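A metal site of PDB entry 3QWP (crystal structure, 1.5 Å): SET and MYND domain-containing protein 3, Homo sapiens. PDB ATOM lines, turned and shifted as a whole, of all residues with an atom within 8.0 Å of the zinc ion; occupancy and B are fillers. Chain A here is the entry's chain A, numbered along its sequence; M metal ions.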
ATOM      1  N   VAL A  49     -17.672  -7.178 -20.964  1.00  0.00           N
ATOM      2  CA  VAL A  49     -18.272  -6.192 -21.870  1.00  0.00           C
ATOM      3  C   VAL A  49     -17.281  -5.815 -22.981  1.00  0.00           C
ATOM      4  O   VAL A  49     -16.061  -5.968 -22.785  1.00  0.00           O
ATOM      5  CB  VAL A  49     -18.725  -4.887 -21.156  1.00  0.00           C
ATOM      6  CG1 VAL A  49     -19.629  -5.252 -19.958  1.00  0.00           C
ATOM      7  CG2 VAL A  49     -17.547  -4.081 -20.656  1.00  0.00           C
ATOM      8  N   CYS A  50     -17.822  -5.321 -24.080  1.00  0.00           N
ATOM      9  CA  CYS A  50     -17.001  -4.911 -25.205  1.00  0.00           C
ATOM     10  C   CYS A  50     -16.087  -3.729 -24.755  1.00  0.00           C
ATOM     11  O   CYS A  50     -16.571  -2.735 -24.168  1.00  0.00           O
ATOM     12  CB  CYS A  50     -17.907  -4.516 -26.332  1.00  0.00           C
ATOM     13  SG  CYS A  50     -17.023  -3.844 -27.772  1.00  0.00           S
ATOM     14  N   ASP A  51     -14.775  -3.872 -24.988  1.00  0.00           N
ATOM     15  CA  ASP A  51     -13.832  -2.771 -24.747  1.00  0.00           C
ATOM     16  C   ASP A  51     -14.339  -1.424 -25.316  1.00  0.00           C
ATOM     17  O   ASP A  51     -14.038  -0.359 -24.757  1.00  0.00           O
ATOM     18  CB  ASP A  51     -12.512  -3.063 -25.446  1.00  0.00           C
ATOM     19  CG  ASP A  51     -11.484  -3.668 -24.530  1.00  0.00           C
ATOM     20  OD1 ASP A  51     -11.742  -4.684 -23.848  1.00  0.00           O
ATOM     21  OD2 ASP A  51     -10.361  -3.146 -24.543  1.00  0.00           O
ATOM     22  N   ARG A  52     -14.934  -1.442 -26.518  1.00  0.00           N
ATOM     23  CA  ARG A  52     -15.307  -0.226 -27.209  1.00  0.00           C
ATOM     24  C   ARG A  52     -16.679   0.249 -26.704  1.00  0.00           C
ATOM     25  O   ARG A  52     -16.806   1.357 -26.179  1.00  0.00           O
ATOM     26  CB  ARG A  52     -15.318  -0.408 -28.764  1.00  0.00           C
ATOM     27  CG  ARG A  52     -15.912   0.822 -29.452  1.00  0.00           C
ATOM     28  CD  ARG A  52     -15.510   0.947 -30.924  1.00  0.00           C
ATOM     29  NE  ARG A  52     -16.162   2.088 -31.572  1.00  0.00           N
ATOM     30  CZ  ARG A  52     -17.458   2.133 -31.906  1.00  0.00           C
ATOM     31  NH1 ARG A  52     -18.266   1.077 -31.694  1.00  0.00           N
ATOM     32  NH2 ARG A  52     -17.942   3.234 -32.467  1.00  0.00           N
ATOM     33  N   CYS A  53     -17.739  -0.560 -26.876  1.00  0.00           N
ATOM     34  CA  CYS A  53     -19.069  -0.008 -26.663  1.00  0.00           C
ATOM     35  C   CYS A  53     -19.581  -0.217 -25.229  1.00  0.00           C
ATOM     36  O   CYS A  53     -20.672   0.311 -24.926  1.00  0.00           O
ATOM     37  CB  CYS A  53     -20.100  -0.566 -27.668  1.00  0.00           C
ATOM     38  SG  CYS A  53     -20.406  -2.325 -27.582  1.00  0.00           S
ATOM     39  N   LEU A  54     -18.843  -1.005 -24.442  1.00  0.00           N
ATOM     40  CA  LEU A  54     -19.146  -1.320 -23.018  1.00  0.00           C
ATOM     41  C   LEU A  54     -20.483  -2.013 -22.854  1.00  0.00           C
ATOM     42  O   LEU A  54     -21.103  -1.967 -21.807  1.00  0.00           O
ATOM     43  CB  LEU A  54     -19.043  -0.055 -22.144  1.00  0.00           C
ATOM     44  CG  LEU A  54     -17.705   0.703 -22.295  1.00  0.00           C
ATOM     45  CD1 LEU A  54     -17.806   1.991 -21.465  1.00  0.00           C
ATOM     46  CD2 LEU A  54     -16.564  -0.156 -21.750  1.00  0.00           C
ATOM     47  N   LEU A  55     -20.859  -2.793 -23.858  1.00  0.00           N
ATOM     48  CA  LEU A  55     -22.063  -3.635 -23.780  1.00  0.00           C
ATOM     49  C   LEU A  55     -21.675  -5.079 -23.477  1.00  0.00           C
ATOM     50  O   LEU A  55     -20.660  -5.590 -23.973  1.00  0.00           O
ATOM     51  CB  LEU A  55     -22.869  -3.570 -25.066  1.00  0.00           C
ATOM     52  CG  LEU A  55     -23.542  -2.269 -25.455  1.00  0.00           C
ATOM     53  CD1 LEU A  55     -24.382  -2.474 -26.681  1.00  0.00           C
ATOM     54  CD2 LEU A  55     -24.437  -1.688 -24.342  1.00  0.00           C
ATOM     55  N   GLY A  56     -22.502  -5.767 -22.700  1.00  0.00           N
ATOM     56  CA  GLY A  56     -22.241  -7.151 -22.358  1.00  0.00           C
ATOM     57  C   GLY A  56     -22.612  -8.067 -23.508  1.00  0.00           C
ATOM     58  O   GLY A  56     -23.456  -7.734 -24.333  1.00  0.00           O
ATOM     59  N   LYS A  57     -21.835  -9.129 -23.663  1.00  0.00           N
ATOM     60  CA  LYS A  57     -22.188 -10.185 -24.607  1.00  0.00           C
ATOM     61  C   LYS A  57     -21.809 -11.537 -24.011  1.00  0.00           C
ATOM     62  O   LYS A  57     -20.929 -11.606 -23.136  1.00  0.00           O
ATOM     63  CB  LYS A  57     -21.494  -9.972 -25.960  1.00  0.00           C
ATOM     64  N   LEU A  60     -17.407 -12.802 -26.466  1.00  0.00           N
ATOM     65  CA  LEU A  60     -16.646 -11.674 -27.014  1.00  0.00           C
ATOM     66  C   LEU A  60     -15.500 -12.189 -27.878  1.00  0.00           C
ATOM     67  O   LEU A  60     -14.966 -13.273 -27.619  1.00  0.00           O
ATOM     68  CB  LEU A  60     -16.071 -10.840 -25.854  1.00  0.00           C
ATOM     69  CG  LEU A  60     -17.099 -10.071 -25.036  1.00  0.00           C
ATOM     70  CD1 LEU A  60     -16.356  -9.381 -23.924  1.00  0.00           C
ATOM     71  CD2 LEU A  60     -17.823  -9.055 -25.900  1.00  0.00           C
ATOM     72  N   LYS A  70     -11.130  -7.107 -25.742  1.00  0.00           N
ATOM     73  CA  LYS A  70     -12.190  -7.959 -26.269  1.00  0.00           C
ATOM     74  C   LYS A  70     -13.388  -7.161 -26.739  1.00  0.00           C
ATOM     75  O   LYS A  70     -13.644  -6.051 -26.246  1.00  0.00           O
ATOM     76  CB  LYS A  70     -12.591  -9.033 -25.242  1.00  0.00           C
ATOM     77  CG  LYS A  70     -11.452  -9.995 -24.918  1.00  0.00           C
ATOM     78  CD  LYS A  70     -11.852 -11.057 -23.920  1.00  0.00           C
ATOM     79  CE  LYS A  70     -10.697 -11.986 -23.587  1.00  0.00           C
ATOM     80  NZ  LYS A  70     -10.881 -12.647 -22.274  1.00  0.00           N
ATOM     81  N   TYR A  71     -14.074  -7.657 -27.756  1.00  0.00           N
ATOM     82  CA  TYR A  71     -15.045  -6.842 -28.463  1.00  0.00           C
ATOM     83  C   TYR A  71     -16.301  -7.616 -28.786  1.00  0.00           C
ATOM     84  O   TYR A  71     -16.266  -8.863 -28.920  1.00  0.00           O
ATOM     85  CB  TYR A  71     -14.436  -6.323 -29.768  1.00  0.00           C
ATOM     86  CG  TYR A  71     -13.154  -5.553 -29.555  1.00  0.00           C
ATOM     87  CD1 TYR A  71     -13.193  -4.202 -29.170  1.00  0.00           C
ATOM     88  CD2 TYR A  71     -11.899  -6.156 -29.733  1.00  0.00           C
ATOM     89  CE1 TYR A  71     -12.014  -3.446 -29.018  1.00  0.00           C
ATOM     90  CE2 TYR A  71     -10.712  -5.407 -29.550  1.00  0.00           C
ATOM     91  CZ  TYR A  71     -10.803  -4.052 -29.193  1.00  0.00           C
ATOM     92  OH  TYR A  71      -9.664  -3.271 -29.015  1.00  0.00           O
ATOM     93  N   CYS A  72     -17.384  -6.873 -28.956  1.00  0.00           N
ATOM     94  CA  CYS A  72     -18.690  -7.409 -29.250  1.00  0.00           C
ATOM     95  C   CYS A  72     -18.815  -7.916 -30.675  1.00  0.00           C
ATOM     96  O   CYS A  72     -19.703  -8.733 -30.994  1.00  0.00           O
ATOM     97  CB  CYS A  72     -19.776  -6.375 -28.958  1.00  0.00           C
ATOM     98  SG  CYS A  72     -20.011  -5.083 -29.968  1.00  0.00           S
ATOM     99  N   SER A  73     -18.000  -7.343 -31.568  1.00  0.00           N
ATOM    100  CA  SER A  73     -18.270  -7.392 -32.995  1.00  0.00           C
ATOM    101  C   SER A  73     -16.994  -7.034 -33.737  1.00  0.00           C
ATOM    102  O   SER A  73     -16.100  -6.314 -33.201  1.00  0.00           O
ATOM    103  CB  SER A  73     -19.408  -6.447 -33.434  1.00  0.00           C
ATOM    104  OG  SER A  73     -19.067  -5.082 -33.066  1.00  0.00           O
ATOM    105  N   ALA A  74     -16.903  -7.504 -34.957  1.00  0.00           N
ATOM    106  CA  ALA A  74     -15.930  -6.943 -35.868  1.00  0.00           C
ATOM    107  C   ALA A  74     -15.928  -5.418 -36.020  1.00  0.00           C
ATOM    108  O   ALA A  74     -14.827  -4.792 -36.049  1.00  0.00           O
ATOM    109  CB  ALA A  74     -16.036  -7.649 -37.223  1.00  0.00           C
ATOM    110  N   LYS A  75     -17.111  -4.786 -36.021  1.00  0.00           N
ATOM    111  CA  LYS A  75     -17.192  -3.351 -36.167  1.00  0.00           C
ATOM    112  C   LYS A  75     -16.478  -2.715 -34.967  1.00  0.00           C
ATOM    113  O   LYS A  75     -15.630  -1.844 -35.126  1.00  0.00           O
ATOM    114  CB  LYS A  75     -18.661  -2.875 -36.226  1.00  0.00           C
ATOM    115  CG  LYS A  75     -18.844  -1.362 -36.233  1.00  0.00           C
ATOM    116  CD  LYS A  75     -20.310  -0.942 -36.041  1.00  0.00           C
ATOM    117  N   CYS A  76     -16.756  -3.215 -33.770  1.00  0.00           N
ATOM    118  CA  CYS A  76     -16.131  -2.550 -32.585  1.00  0.00           C
ATOM    119  C   CYS A  76     -14.630  -2.779 -32.528  1.00  0.00           C
ATOM    120  O   CYS A  76     -13.880  -1.805 -32.271  1.00  0.00           O
ATOM    121  CB  CYS A  76     -16.771  -3.020 -31.289  1.00  0.00           C
ATOM    122  SG  CYS A  76     -18.326  -2.085 -30.869  1.00  0.00           S
ATOM    123  N   GLN A  77     -14.166  -4.008 -32.849  1.00  0.00           N
ATOM    124  CA  GLN A  77     -12.730  -4.319 -32.783  1.00  0.00           C
ATOM    125  C   GLN A  77     -11.984  -3.413 -33.799  1.00  0.00           C
ATOM    126  O   GLN A  77     -10.922  -2.829 -33.524  1.00  0.00           O
ATOM    127  CB  GLN A  77     -12.486  -5.775 -33.113  1.00  0.00           C
ATOM    128  CG  GLN A  77     -11.019  -6.098 -33.111  1.00  0.00           C
ATOM    129  CD  GLN A  77     -10.704  -7.559 -33.198  1.00  0.00           C
ATOM    130  OE1 GLN A  77     -11.601  -8.420 -33.036  1.00  0.00           O
ATOM    131  NE2 GLN A  77      -9.423  -7.878 -33.374  1.00  0.00           N
HETATM  132 ZN    ZN M   1     -18.997  -3.297 -29.014  1.00  0.00          ZN
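Of the 18 residues printed, 4 come within 4 Å of the zinc ion.
SG of Cys 53 binds the zinc ion, at 2.2 Å. SG of Cys 72 is bound to the zinc ion (2.3 Å). The zinc ion is bound by SG of Cys 76, at 2.3 Å. SG of Cys 50 is bound to the zinc ion (2.4 Å). The zinc ion has four donor atoms within binding distance.
The side-chain sulfur (SG) of Cys 53 sits close to the backbone NH (N) of Leu 55 (3.8 Å). The side-chain hydroxyl (OG) of Ser 73 sits close to the side-chain sulfur (SG) of Cys 72. N of Cys 76 is in hydrogen-bond range of OG of Ser 73, 3.1 Å away. The side-chain sulfur of Cys 76 sits close to the guanidinium group of Arg 52, at 3.3 Å. N of Arg 52 sits close to SG of Cys 50 (3.4 Å). The backbone NH (N) of Cys 50 sits at hydrogen-bond distance from the backbone carbonyl oxygen (O) of Leu 55, 2.9 Å away.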
